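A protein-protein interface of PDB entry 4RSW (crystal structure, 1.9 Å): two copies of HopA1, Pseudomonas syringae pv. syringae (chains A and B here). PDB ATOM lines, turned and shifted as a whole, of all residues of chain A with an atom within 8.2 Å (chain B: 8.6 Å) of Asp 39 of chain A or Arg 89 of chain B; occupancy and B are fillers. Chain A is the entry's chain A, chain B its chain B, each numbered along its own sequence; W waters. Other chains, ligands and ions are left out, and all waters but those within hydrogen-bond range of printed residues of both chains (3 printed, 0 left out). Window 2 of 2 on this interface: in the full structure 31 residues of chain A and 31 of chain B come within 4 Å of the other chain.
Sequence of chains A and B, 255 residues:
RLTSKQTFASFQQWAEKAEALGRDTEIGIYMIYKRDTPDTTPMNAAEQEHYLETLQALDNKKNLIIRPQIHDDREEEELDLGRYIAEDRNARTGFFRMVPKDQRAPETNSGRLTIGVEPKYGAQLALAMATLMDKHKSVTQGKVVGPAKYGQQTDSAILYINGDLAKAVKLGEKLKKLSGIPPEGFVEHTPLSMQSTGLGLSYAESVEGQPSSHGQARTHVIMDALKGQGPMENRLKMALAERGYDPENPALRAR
Of the 18 printed residues of chain A, 6 touch a printed residue of chain B. Along chain A the printed residues that touch a printed residue of chain B span positions 35 to 152. Hydrophobic or aromatic side chains of chain B within 4 Å of the printed part of chain A: Ala 148.
OE1 of Gln 152 of chain A sits close to O of Ala 148 of chain B, 3.2 Å away. The side-chain hydroxyl (OG1) of Thr 93 of chain B is in hydrogen-bond range of the side-chain hydroxyl (OG1) of Thr 37 of chain A (2.6 Å). The backbone carbonyl oxygen of Arg 35 of chain A lies close to the side-chain amide oxygen of Asn 90 of chain B, at 3.2 Å. N of Thr 37 of chain A is in hydrogen-bond range of OD1 of Asn 90 of chain B, 2.9 Å away. The guanidinium group of Arg 89 of chain B is in salt-bridge range of the side-chain carboxylate of Asp 39 of chain A, at 3.5 Å. O of Thr 40 of chain A lies within hydrogen-bond range of NH2 of Arg 89 of chain B (2.7 Å).
Among the printed residues, pairs that only touch across the chains: Asp 36 of chain A with Asn 90 of chain B (3.9 Å), Thr 37 of chain A with Arg 89 of chain B (3.9 Å) and Gln 152 of chain A with Thr 93 of chain B (3.5 Å).
No position is printed for both chains.
Asp 39 of chain A touches one residue of chain B. Arg 89 of chain B touches three residues of chain A. Of the printed residues of chain B, Thr 40 of chain A touches Arg 89. Printed residues of chain A within 4 Å of Ala 148 of chain B: Gln 152 (3.2 Å). Of the printed residues of chain B, Arg 35 of chain A touches Asn 90. Printed residues of chain B within 4 Å of Asp 36 of chain A: Asn 90. Of the printed residues of chain A, Thr 93 of chain B touches Thr 37 and Gln 152. The nearest printed residue of chain B that does not touch Asp 36 of chain A is Thr 93 of chain B (6.2 Å).
Water W2 lies within hydrogen-bond range of O of Arg 35 of chain A, OG1 of Thr 93 of chain B and N of Gly 94 of chain B. Water W3 lies within hydrogen-bond range of the backbone carbonyl oxygen (O) of Gln 152 of chain A (2.9 Å), the side-chain hydroxyl (OG1) of Thr 37 of chain A (3.0 Å), the backbone carbonyl oxygen (O) of Arg 35 of chain A (3.1 Å) and the side-chain hydroxyl (OG1) of Thr 93 of chain B (3.2 Å). Water W1 lies within hydrogen-bond range of ND2 of Asn 90 of chain B and OD1 of Asp 36 of chain A.
The side-chain carboxylate (OD1) of Asp 88 of chain B is in hydrogen-bond range of the backbone NH (N) of Asn 90 of chain B (3.0 Å). The side-chain hydroxyl (OG1) of Thr 37 of chain A sits at hydrogen-bond distance from the backbone carbonyl oxygen (O) of Arg 35 of chain A (3.0 Å). The backbone carbonyl oxygen of Asn 90 of chain B is in hydrogen-bond range of the side-chain hydroxyl of Thr 93 of chain B, 3.5 Å away. The backbone carbonyl oxygen (O) of Arg 92 of chain B sits at hydrogen-bond distance from the backbone NH (N) of Ala 148 of chain B (2.9 Å). The side-chain hydroxyl (OG1) of Thr 40 of chain A sits at hydrogen-bond distance from the backbone carbonyl oxygen (O) of Gly 151 of chain A, at 2.7 Å. The backbone carbonyl oxygen of Asn 90 of chain B sits close to the side-chain hydroxyl of Tyr 84 of chain B.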
ATOM      1  N   ARG A  35      10.762 -18.238  20.614  1.00  0.00           N
ATOM      2  CA  ARG A  35       9.449 -18.891  20.550  1.00  0.00           C
ATOM      3  C   ARG A  35       9.507 -20.356  20.105  1.00  0.00           C
ATOM      4  O   ARG A  35       8.480 -21.010  19.850  1.00  0.00           O
ATOM      5  CB  ARG A  35       8.506 -18.101  19.641  1.00  0.00           C
ATOM      6  CG  ARG A  35       8.189 -16.728  20.162  1.00  0.00           C
ATOM      7  CD  ARG A  35       7.234 -15.978  19.223  1.00  0.00           C
ATOM      8  NE  ARG A  35       6.997 -14.636  19.731  1.00  0.00           N
ATOM      9  CZ  ARG A  35       6.326 -13.687  19.094  1.00  0.00           C
ATOM     10  NH1 ARG A  35       5.826 -13.923  17.899  1.00  0.00           N
ATOM     11  NH2 ARG A  35       6.165 -12.490  19.654  1.00  0.00           N
ATOM     12  N   ASP A  36      10.723 -20.860  20.015  1.00  0.00           N
ATOM     13  CA  ASP A  36      10.991 -22.250  19.699  1.00  0.00           C
ATOM     14  C   ASP A  36      10.526 -23.103  20.889  1.00  0.00           C
ATOM     15  O   ASP A  36      11.213 -23.189  21.908  1.00  0.00           O
ATOM     16  CB  ASP A  36      12.497 -22.334  19.474  1.00  0.00           C
ATOM     17  CG  ASP A  36      13.006 -23.740  19.273  1.00  0.00           C
ATOM     18  OD1 ASP A  36      12.274 -24.602  18.731  1.00  0.00           O
ATOM     19  OD2 ASP A  36      14.182 -23.955  19.642  1.00  0.00           O
ATOM     20  N   THR A  37       9.360 -23.735  20.763  1.00  0.00           N
ATOM     21  CA  THR A  37       8.672 -24.338  21.915  1.00  0.00           C
ATOM     22  C   THR A  37       8.994 -25.812  22.135  1.00  0.00           C
ATOM     23  O   THR A  37       8.822 -26.615  21.231  1.00  0.00           O
ATOM     24  CB  THR A  37       7.140 -24.232  21.740  1.00  0.00           C
ATOM     25  OG1 THR A  37       6.778 -22.859  21.540  1.00  0.00           O
ATOM     26  CG2 THR A  37       6.411 -24.779  22.958  1.00  0.00           C
ATOM     27  N   PRO A  38       9.447 -26.175  23.347  1.00  0.00           N
ATOM     28  CA  PRO A  38       9.664 -27.590  23.677  1.00  0.00           C
ATOM     29  C   PRO A  38       8.342 -28.301  23.950  1.00  0.00           C
ATOM     30  O   PRO A  38       7.372 -27.634  24.301  1.00  0.00           O
ATOM     31  CB  PRO A  38      10.476 -27.515  24.968  1.00  0.00           C
ATOM     32  CG  PRO A  38      10.028 -26.254  25.607  1.00  0.00           C
ATOM     33  CD  PRO A  38       9.834 -25.289  24.460  1.00  0.00           C
ATOM     34  N   ASP A  39       8.301 -29.625  23.799  1.00  0.00           N
ATOM     35  CA  ASP A  39       7.085 -30.389  24.100  1.00  0.00           C
ATOM     36  C   ASP A  39       6.947 -30.595  25.605  1.00  0.00           C
ATOM     37  O   ASP A  39       7.670 -31.396  26.190  1.00  0.00           O
ATOM     38  CB  ASP A  39       7.097 -31.745  23.383  1.00  0.00           C
ATOM     39  CG  ASP A  39       5.695 -32.310  23.175  1.00  0.00           C
ATOM     40  OD1 ASP A  39       4.785 -31.961  23.962  1.00  0.00           O
ATOM     41  OD2 ASP A  39       5.500 -33.103  22.221  1.00  0.00           O
ATOM     42  N   THR A  40       6.031 -29.860  26.231  1.00  0.00           N
ATOM     43  CA  THR A  40       5.836 -29.931  27.684  1.00  0.00           C
ATOM     44  C   THR A  40       4.351 -29.967  28.049  1.00  0.00           C
ATOM     45  O   THR A  40       3.501 -29.599  27.241  1.00  0.00           O
ATOM     46  CB  THR A  40       6.458 -28.711  28.405  1.00  0.00           C
ATOM     47  OG1 THR A  40       5.834 -27.508  27.937  1.00  0.00           O
ATOM     48  CG2 THR A  40       7.953 -28.626  28.170  1.00  0.00           C
ATOM     49  N   THR A  41       4.048 -30.412  29.267  1.00  0.00           N
ATOM     50  CA  THR A  41       2.685 -30.361  29.796  1.00  0.00           C
ATOM     51  C   THR A  41       2.610 -29.276  30.853  1.00  0.00           C
ATOM     52  O   THR A  41       3.321 -29.342  31.859  1.00  0.00           O
ATOM     53  CB  THR A  41       2.276 -31.697  30.451  1.00  0.00           C
ATOM     54  OG1 THR A  41       2.300 -32.746  29.475  1.00  0.00           O
ATOM     55  CG2 THR A  41       0.881 -31.583  31.050  1.00  0.00           C
ATOM     56  N   PRO A  42       1.734 -28.279  30.643  1.00  0.00           N
ATOM     57  CA  PRO A  42       1.683 -27.111  31.528  1.00  0.00           C
ATOM     58  C   PRO A  42       1.258 -27.465  32.942  1.00  0.00           C
ATOM     59  O   PRO A  42       0.653 -28.513  33.158  1.00  0.00           O
ATOM     60  CB  PRO A  42       0.615 -26.219  30.871  1.00  0.00           C
ATOM     61  CG  PRO A  42       0.549 -26.674  29.446  1.00  0.00           C
ATOM     62  CD  PRO A  42       0.803 -28.151  29.506  1.00  0.00           C
ATOM     63  N   VAL A 117      13.004 -28.802  32.527  1.00  0.00           N
ATOM     64  CA  VAL A 117      12.213 -29.845  33.190  1.00  0.00           C
ATOM     65  C   VAL A 117      10.728 -29.669  32.857  1.00  0.00           C
ATOM     66  O   VAL A 117      10.287 -28.563  32.510  1.00  0.00           O
ATOM     67  CB  VAL A 117      12.369 -29.801  34.730  1.00  0.00           C
ATOM     68  CG1 VAL A 117      13.803 -30.091  35.144  1.00  0.00           C
ATOM     69  CG2 VAL A 117      11.920 -28.463  35.285  1.00  0.00           C
ATOM     70  N   GLU A 118       9.956 -30.751  32.955  1.00  0.00           N
ATOM     71  CA  GLU A 118       8.505 -30.648  32.815  1.00  0.00           C
ATOM     72  C   GLU A 118       8.015 -29.662  33.867  1.00  0.00           C
ATOM     73  O   GLU A 118       8.526 -29.650  34.989  1.00  0.00           O
ATOM     74  CB  GLU A 118       7.842 -32.024  32.992  1.00  0.00           C
ATOM     75  CG  GLU A 118       8.048 -32.981  31.803  1.00  0.00           C
ATOM     76  CD  GLU A 118       7.083 -32.712  30.655  1.00  0.00           C
ATOM     77  OE1 GLU A 118       6.149 -31.911  30.843  1.00  0.00           O
ATOM     78  OE2 GLU A 118       7.247 -33.306  29.564  1.00  0.00           O
ATOM     79  N   PRO A 119       7.049 -28.799  33.501  1.00  0.00           N
ATOM     80  CA  PRO A 119       6.623 -27.720  34.402  1.00  0.00           C
ATOM     81  C   PRO A 119       6.194 -28.183  35.798  1.00  0.00           C
ATOM     82  O   PRO A 119       6.364 -27.418  36.744  1.00  0.00           O
ATOM     83  CB  PRO A 119       5.438 -27.092  33.657  1.00  0.00           C
ATOM     84  CG  PRO A 119       5.742 -27.356  32.202  1.00  0.00           C
ATOM     85  CD  PRO A 119       6.383 -28.722  32.187  1.00  0.00           C
ATOM     86  N   GLY A 151       7.776 -23.752  30.562  1.00  0.00           N
ATOM     87  CA  GLY A 151       7.808 -24.739  29.499  1.00  0.00           C
ATOM     88  C   GLY A 151       7.228 -24.337  28.154  1.00  0.00           C
ATOM     89  O   GLY A 151       7.077 -25.187  27.277  1.00  0.00           O
ATOM     90  N   GLN A 152       6.929 -23.054  27.957  1.00  0.00           N
ATOM     91  CA  GLN A 152       6.198 -22.648  26.750  1.00  0.00           C
ATOM     92  C   GLN A 152       6.986 -21.747  25.803  1.00  0.00           C
ATOM     93  O   GLN A 152       6.451 -21.205  24.842  1.00  0.00           O
ATOM     94  CB  GLN A 152       4.838 -22.053  27.130  1.00  0.00           C
ATOM     95  CG  GLN A 152       3.931 -23.131  27.770  1.00  0.00           C
ATOM     96  CD  GLN A 152       2.559 -22.621  28.172  1.00  0.00           C
ATOM     97  OE1 GLN A 152       2.146 -21.524  27.786  1.00  0.00           O
ATOM     98  NE2 GLN A 152       1.839 -23.427  28.955  1.00  0.00           N
ATOM     99  N   GLN A 153       8.273 -21.602  26.081  1.00  0.00           N
ATOM    100  CA  GLN A 153       9.173 -20.915  25.163  1.00  0.00           C
ATOM    101  C   GLN A 153      10.529 -21.592  25.320  1.00  0.00           C
ATOM    102  O   GLN A 153      10.627 -22.594  26.023  1.00  0.00           O
ATOM    103  CB  GLN A 153       9.238 -19.423  25.433  1.00  0.00           C
ATOM    104  CG  GLN A 153       9.686 -19.026  26.813  1.00  0.00           C
ATOM    105  CD  GLN A 153       8.594 -19.253  27.842  1.00  0.00           C
ATOM    106  OE1 GLN A 153       7.439 -18.925  27.598  1.00  0.00           O
ATOM    107  NE2 GLN A 153       8.950 -19.847  28.979  1.00  0.00           N
ATOM    108  N   PHE A 186      13.059 -34.421  33.014  1.00  0.00           N
ATOM    109  CA  PHE A 186      13.868 -33.490  32.223  1.00  0.00           C
ATOM    110  C   PHE A 186      13.445 -33.515  30.762  1.00  0.00           C
ATOM    111  O   PHE A 186      13.044 -34.565  30.255  1.00  0.00           O
ATOM    112  CB  PHE A 186      15.365 -33.799  32.369  1.00  0.00           C
ATOM    113  CG  PHE A 186      15.926 -33.404  33.709  1.00  0.00           C
ATOM    114  CD1 PHE A 186      16.442 -32.126  33.910  1.00  0.00           C
ATOM    115  CD2 PHE A 186      15.905 -34.296  34.777  1.00  0.00           C
ATOM    116  CE1 PHE A 186      16.942 -31.751  35.142  1.00  0.00           C
ATOM    117  CE2 PHE A 186      16.404 -33.935  36.015  1.00  0.00           C
ATOM    118  CZ  PHE A 186      16.927 -32.656  36.203  1.00  0.00           C
ATOM    119  N   VAL A 187      13.542 -32.359  30.096  1.00  0.00           N
ATOM    120  CA  VAL A 187      13.012 -32.174  28.746  1.00  0.00           C
ATOM    121  C   VAL A 187      14.108 -32.124  27.692  1.00  0.00           C
ATOM    122  O   VAL A 187      15.042 -31.320  27.793  1.00  0.00           O
ATOM    123  CB  VAL A 187      12.205 -30.844  28.648  1.00  0.00           C
ATOM    124  CG1 VAL A 187      11.795 -30.567  27.209  1.00  0.00           C
ATOM    125  CG2 VAL A 187      11.000 -30.869  29.577  1.00  0.00           C
ATOM    126  N   GLU A 188      14.001 -32.966  26.670  1.00  0.00           N
ATOM    127  CA  GLU A 188      14.976 -32.939  25.591  1.00  0.00           C
ATOM    128  C   GLU A 188      14.751 -31.715  24.714  1.00  0.00           C
ATOM    129  O   GLU A 188      13.860 -31.703  23.854  1.00  0.00           O
ATOM    130  CB  GLU A 188      14.910 -34.203  24.745  1.00  0.00           C
ATOM    131  CG  GLU A 188      15.951 -34.251  23.632  1.00  0.00           C
ATOM    132  CD  GLU A 188      17.378 -34.355  24.154  1.00  0.00           C
ATOM    133  OE1 GLU A 188      17.701 -35.363  24.832  1.00  0.00           O
ATOM    134  OE2 GLU A 188      18.189 -33.433  23.886  1.00  0.00           O
ATOM    135  N   HIS A 189      15.568 -30.688  24.931  1.00  0.00           N
ATOM    136  CA  HIS A 189      15.453 -29.448  24.167  1.00  0.00           C
ATOM    137  C   HIS A 189      16.722 -28.622  24.334  1.00  0.00           C
ATOM    138  O   HIS A 189      17.177 -28.379  25.461  1.00  0.00           O
ATOM    139  CB  HIS A 189      14.248 -28.636  24.654  1.00  0.00           C
ATOM    140  CG  HIS A 189      14.110 -27.292  23.996  1.00  0.00           C
ATOM    141  ND1 HIS A 189      13.570 -27.129  22.737  1.00  0.00           N
ATOM    142  CD2 HIS A 189      14.434 -26.049  24.428  1.00  0.00           C
ATOM    143  CE1 HIS A 189      13.575 -25.844  22.420  1.00  0.00           C
ATOM    144  NE2 HIS A 189      14.099 -25.168  23.428  1.00  0.00           N
ATOM    145  N   GLN B  48      -8.675 -25.180  24.692  1.00  0.00           N
ATOM    146  CA  GLN B  48      -7.515 -25.051  23.799  1.00  0.00           C
ATOM    147  C   GLN B  48      -7.668 -25.891  22.527  1.00  0.00           C
ATOM    148  O   GLN B  48      -7.355 -25.441  21.432  1.00  0.00           O
ATOM    149  CB  GLN B  48      -6.212 -25.408  24.516  1.00  0.00           C
ATOM    150  CG  GLN B  48      -5.796 -24.413  25.586  1.00  0.00           C
ATOM    151  CD  GLN B  48      -4.348 -24.587  26.000  1.00  0.00           C
ATOM    152  OE1 GLN B  48      -3.509 -25.014  25.199  1.00  0.00           O
ATOM    153  NE2 GLN B  48      -4.041 -24.258  27.254  1.00  0.00           N
ATOM    154  N   LEU B  52      -7.920 -24.597  18.609  1.00  0.00           N
ATOM    155  CA  LEU B  52      -7.141 -25.084  17.485  1.00  0.00           C
ATOM    156  C   LEU B  52      -8.066 -25.678  16.424  1.00  0.00           C
ATOM    157  O   LEU B  52      -7.835 -25.509  15.230  1.00  0.00           O
ATOM    158  CB  LEU B  52      -6.071 -26.074  17.945  1.00  0.00           C
ATOM    159  CG  LEU B  52      -4.922 -25.395  18.708  1.00  0.00           C
ATOM    160  CD1 LEU B  52      -3.987 -26.416  19.347  1.00  0.00           C
ATOM    161  CD2 LEU B  52      -4.141 -24.473  17.778  1.00  0.00           C
ATOM    162  N   ILE B  70       5.632 -18.726  11.584  1.00  0.00           N
ATOM    163  CA  ILE B  70       6.890 -19.456  11.374  1.00  0.00           C
ATOM    164  C   ILE B  70       6.935 -20.131   9.981  1.00  0.00           C
ATOM    165  O   ILE B  70       7.968 -20.674   9.572  1.00  0.00           O
ATOM    166  CB  ILE B  70       7.179 -20.440  12.556  1.00  0.00           C
ATOM    167  CG1 ILE B  70       8.629 -20.949  12.532  1.00  0.00           C
ATOM    168  CG2 ILE B  70       6.199 -21.592  12.558  1.00  0.00           C
ATOM    169  CD1 ILE B  70       9.654 -19.842  12.487  1.00  0.00           C
ATOM    170  N   ARG B  83      -1.091 -30.631   9.548  1.00  0.00           N
ATOM    171  CA  ARG B  83       0.135 -31.265  10.004  1.00  0.00           C
ATOM    172  C   ARG B  83       0.834 -30.423  11.077  1.00  0.00           C
ATOM    173  O   ARG B  83       1.317 -30.960  12.078  1.00  0.00           O
ATOM    174  CB  ARG B  83       1.055 -31.505   8.810  1.00  0.00           C
ATOM    175  CG  ARG B  83       2.286 -32.326   9.119  1.00  0.00           C
ATOM    176  CD  ARG B  83       2.819 -32.977   7.863  1.00  0.00           C
ATOM    177  NE  ARG B  83       4.261 -33.195   7.934  1.00  0.00           N
ATOM    178  CZ  ARG B  83       4.953 -33.882   7.031  1.00  0.00           C
ATOM    179  NH1 ARG B  83       4.331 -34.429   5.998  1.00  0.00           N
ATOM    180  NH2 ARG B  83       6.265 -34.030   7.167  1.00  0.00           N
ATOM    181  N   TYR B  84       0.873 -29.106  10.870  1.00  0.00           N
ATOM    182  CA  TYR B  84       1.460 -28.179  11.846  1.00  0.00           C
ATOM    183  C   TYR B  84       0.790 -28.329  13.211  1.00  0.00           C
ATOM    184  O   TYR B  84       1.459 -28.502  14.234  1.00  0.00           O
ATOM    185  CB  TYR B  84       1.358 -26.735  11.320  1.00  0.00           C
ATOM    186  CG  TYR B  84       1.884 -25.644  12.246  1.00  0.00           C
ATOM    187  CD1 TYR B  84       3.243 -25.405  12.370  1.00  0.00           C
ATOM    188  CD2 TYR B  84       1.010 -24.839  12.972  1.00  0.00           C
ATOM    189  CE1 TYR B  84       3.730 -24.405  13.212  1.00  0.00           C
ATOM    190  CE2 TYR B  84       1.480 -23.832  13.807  1.00  0.00           C
ATOM    191  CZ  TYR B  84       2.840 -23.625  13.930  1.00  0.00           C
ATOM    192  OH  TYR B  84       3.301 -22.624  14.768  1.00  0.00           O
ATOM    193  N   ILE B  85      -0.538 -28.299  13.223  1.00  0.00           N
ATOM    194  CA  ILE B  85      -1.295 -28.386  14.470  1.00  0.00           C
ATOM    195  C   ILE B  85      -1.119 -29.731  15.180  1.00  0.00           C
ATOM    196  O   ILE B  85      -1.000 -29.784  16.406  1.00  0.00           O
ATOM    197  CB  ILE B  85      -2.796 -28.102  14.225  1.00  0.00           C
ATOM    198  CG1 ILE B  85      -3.010 -26.603  13.993  1.00  0.00           C
ATOM    199  CG2 ILE B  85      -3.631 -28.547  15.402  1.00  0.00           C
ATOM    200  CD1 ILE B  85      -4.428 -26.219  13.615  1.00  0.00           C
ATOM    201  N   ALA B  86      -1.101 -30.814  14.407  1.00  0.00           N
ATOM    202  CA  ALA B  86      -0.926 -32.148  14.977  1.00  0.00           C
ATOM    203  C   ALA B  86       0.509 -32.408  15.424  1.00  0.00           C
ATOM    204  O   ALA B  86       0.733 -33.100  16.420  1.00  0.00           O
ATOM    205  CB  ALA B  86      -1.354 -33.204  13.982  1.00  0.00           C
ATOM    206  N   GLU B  87       1.480 -31.862  14.692  1.00  0.00           N
ATOM    207  CA  GLU B  87       2.876 -32.265  14.889  1.00  0.00           C
ATOM    208  C   GLU B  87       3.844 -31.216  15.439  1.00  0.00           C
ATOM    209  O   GLU B  87       4.916 -31.567  15.928  1.00  0.00           O
ATOM    210  CB  GLU B  87       3.458 -32.787  13.577  1.00  0.00           C
ATOM    211  CG  GLU B  87       2.703 -33.930  12.941  1.00  0.00           C
ATOM    212  CD  GLU B  87       3.351 -34.353  11.640  1.00  0.00           C
ATOM    213  OE1 GLU B  87       4.245 -33.613  11.164  1.00  0.00           O
ATOM    214  OE2 GLU B  87       2.980 -35.416  11.095  1.00  0.00           O
ATOM    215  N   ASP B  88       3.507 -29.939  15.330  1.00  0.00           N
ATOM    216  CA  ASP B  88       4.470 -28.900  15.695  1.00  0.00           C
ATOM    217  C   ASP B  88       4.015 -28.243  16.995  1.00  0.00           C
ATOM    218  O   ASP B  88       2.932 -27.678  17.045  1.00  0.00           O
ATOM    219  CB  ASP B  88       4.599 -27.871  14.560  1.00  0.00           C
ATOM    220  CG  ASP B  88       5.841 -27.000  14.684  1.00  0.00           C
ATOM    221  OD1 ASP B  88       6.270 -26.733  15.822  1.00  0.00           O
ATOM    222  OD2 ASP B  88       6.389 -26.571  13.643  1.00  0.00           O
ATOM    223  N   ARG B  89       4.821 -28.328  18.053  1.00  0.00           N
ATOM    224  CA  ARG B  89       4.404 -27.765  19.340  1.00  0.00           C
ATOM    225  C   ARG B  89       4.333 -26.242  19.324  1.00  0.00           C
ATOM    226  O   ARG B  89       3.777 -25.633  20.238  1.00  0.00           O
ATOM    227  CB  ARG B  89       5.306 -28.238  20.480  1.00  0.00           C
ATOM    228  CG  ARG B  89       4.918 -29.608  21.005  1.00  0.00           C
ATOM    229  CD  ARG B  89       3.416 -29.667  21.268  1.00  0.00           C
ATOM    230  NE  ARG B  89       3.062 -29.188  22.602  1.00  0.00           N
ATOM    231  CZ  ARG B  89       2.671 -29.983  23.595  1.00  0.00           C
ATOM    232  NH1 ARG B  89       2.581 -31.291  23.394  1.00  0.00           N
ATOM    233  NH2 ARG B  89       2.363 -29.481  24.785  1.00  0.00           N
ATOM    234  N   ASN B  90       4.894 -25.631  18.288  1.00  0.00           N
ATOM    235  CA  ASN B  90       4.801 -24.187  18.139  1.00  0.00           C
ATOM    236  C   ASN B  90       3.343 -23.767  17.930  1.00  0.00           C
ATOM    237  O   ASN B  90       2.973 -22.630  18.200  1.00  0.00           O
ATOM    238  CB  ASN B  90       5.670 -23.716  16.980  1.00  0.00           C
ATOM    239  CG  ASN B  90       7.159 -23.750  17.311  1.00  0.00           C
ATOM    240  OD1 ASN B  90       7.550 -23.709  18.475  1.00  0.00           O
ATOM    241  ND2 ASN B  90       7.991 -23.829  16.286  1.00  0.00           N
ATOM    242  N   ALA B  91       2.514 -24.693  17.461  1.00  0.00           N
ATOM    243  CA  ALA B  91       1.098 -24.398  17.242  1.00  0.00           C
ATOM    244  C   ALA B  91       0.385 -24.024  18.532  1.00  0.00           C
ATOM    245  O   ALA B  91      -0.629 -23.325  18.508  1.00  0.00           O
ATOM    246  CB  ALA B  91       0.405 -25.584  16.563  1.00  0.00           C
ATOM    247  N   ARG B  92       0.911 -24.470  19.668  1.00  0.00           N
ATOM    248  CA  ARG B  92       0.295 -24.121  20.934  1.00  0.00           C
ATOM    249  C   ARG B  92       0.616 -22.685  21.358  1.00  0.00           C
ATOM    250  O   ARG B  92      -0.100 -22.115  22.167  1.00  0.00           O
ATOM    251  CB  ARG B  92       0.723 -25.095  22.036  1.00  0.00           C
ATOM    252  CG  ARG B  92       0.656 -26.555  21.635  1.00  0.00           C
ATOM    253  CD  ARG B  92      -0.770 -26.961  21.294  1.00  0.00           C
ATOM    254  NE  ARG B  92      -1.629 -26.958  22.479  1.00  0.00           N
ATOM    255  CZ  ARG B  92      -2.614 -27.830  22.692  1.00  0.00           C
ATOM    256  NH1 ARG B  92      -2.869 -28.777  21.795  1.00  0.00           N
ATOM    257  NH2 ARG B  92      -3.345 -27.760  23.801  1.00  0.00           N
ATOM    258  N   THR B  93       1.677 -22.097  20.806  1.00  0.00           N
ATOM    259  CA  THR B  93       2.213 -20.858  21.370  1.00  0.00           C
ATOM    260  C   THR B  93       2.424 -19.729  20.362  1.00  0.00           C
ATOM    261  O   THR B  93       2.376 -18.551  20.731  1.00  0.00           O
ATOM    262  CB  THR B  93       3.553 -21.124  22.114  1.00  0.00           C
ATOM    263  OG1 THR B  93       4.446 -21.810  21.239  1.00  0.00           O
ATOM    264  CG2 THR B  93       3.325 -21.976  23.363  1.00  0.00           C
ATOM    265  N   GLY B  94       2.657 -20.082  19.105  1.00  0.00           N
ATOM    266  CA  GLY B  94       3.010 -19.109  18.091  1.00  0.00           C
ATOM    267  C   GLY B  94       1.810 -18.338  17.575  1.00  0.00           C
ATOM    268  O   GLY B  94       0.656 -18.725  17.820  1.00  0.00           O
ATOM    269  N   PHE B  96      -0.678 -17.129  14.585  1.00  0.00           N
ATOM    270  CA  PHE B  96      -1.216 -17.571  13.302  1.00  0.00           C
ATOM    271  C   PHE B  96      -1.668 -16.346  12.529  1.00  0.00           C
ATOM    272  O   PHE B  96      -2.344 -15.496  13.100  1.00  0.00           O
ATOM    273  CB  PHE B  96      -2.456 -18.459  13.522  1.00  0.00           C
ATOM    274  CG  PHE B  96      -2.168 -19.782  14.195  1.00  0.00           C
ATOM    275  CD1 PHE B  96      -2.068 -19.876  15.573  1.00  0.00           C
ATOM    276  CD2 PHE B  96      -2.003 -20.930  13.441  1.00  0.00           C
ATOM    277  CE1 PHE B  96      -1.793 -21.104  16.188  1.00  0.00           C
ATOM    278  CE2 PHE B  96      -1.731 -22.157  14.054  1.00  0.00           C
ATOM    279  CZ  PHE B  96      -1.641 -22.240  15.419  1.00  0.00           C
ATOM    280  N   GLY B 146      -1.313 -18.606  19.724  1.00  0.00           N
ATOM    281  CA  GLY B 146      -1.635 -19.974  20.085  1.00  0.00           C
ATOM    282  C   GLY B 146      -2.344 -20.057  21.418  1.00  0.00           C
ATOM    283  O   GLY B 146      -2.188 -19.183  22.275  1.00  0.00           O
ATOM    284  N   PRO B 147      -3.125 -21.122  21.612  1.00  0.00           N
ATOM    285  CA  PRO B 147      -4.011 -21.200  22.780  1.00  0.00           C
ATOM    286  C   PRO B 147      -3.290 -21.169  24.125  1.00  0.00           C
ATOM    287  O   PRO B 147      -3.828 -20.620  25.079  1.00  0.00           O
ATOM    288  CB  PRO B 147      -4.729 -22.546  22.591  1.00  0.00           C
ATOM    289  CG  PRO B 147      -3.863 -23.321  21.627  1.00  0.00           C
ATOM    290  CD  PRO B 147      -3.253 -22.294  20.729  1.00  0.00           C
ATOM    291  N   ALA B 148      -2.090 -21.740  24.207  1.00  0.00           N
ATOM    292  CA  ALA B 148      -1.382 -21.815  25.486  1.00  0.00           C
ATOM    293  C   ALA B 148      -0.925 -20.443  25.976  1.00  0.00           C
ATOM    294  O   ALA B 148      -0.702 -20.257  27.159  1.00  0.00           O
ATOM    295  CB  ALA B 148      -0.203 -22.756  25.390  1.00  0.00           C
HETATM  296  O   HOH W   1      10.904 -23.829  16.271  1.00  0.00           O
HETATM  297  O   HOH W   2       6.014 -20.368  18.993  1.00  0.00           O
HETATM  298  O   HOH W   3       6.855 -19.936  22.310  1.00  0.00           O
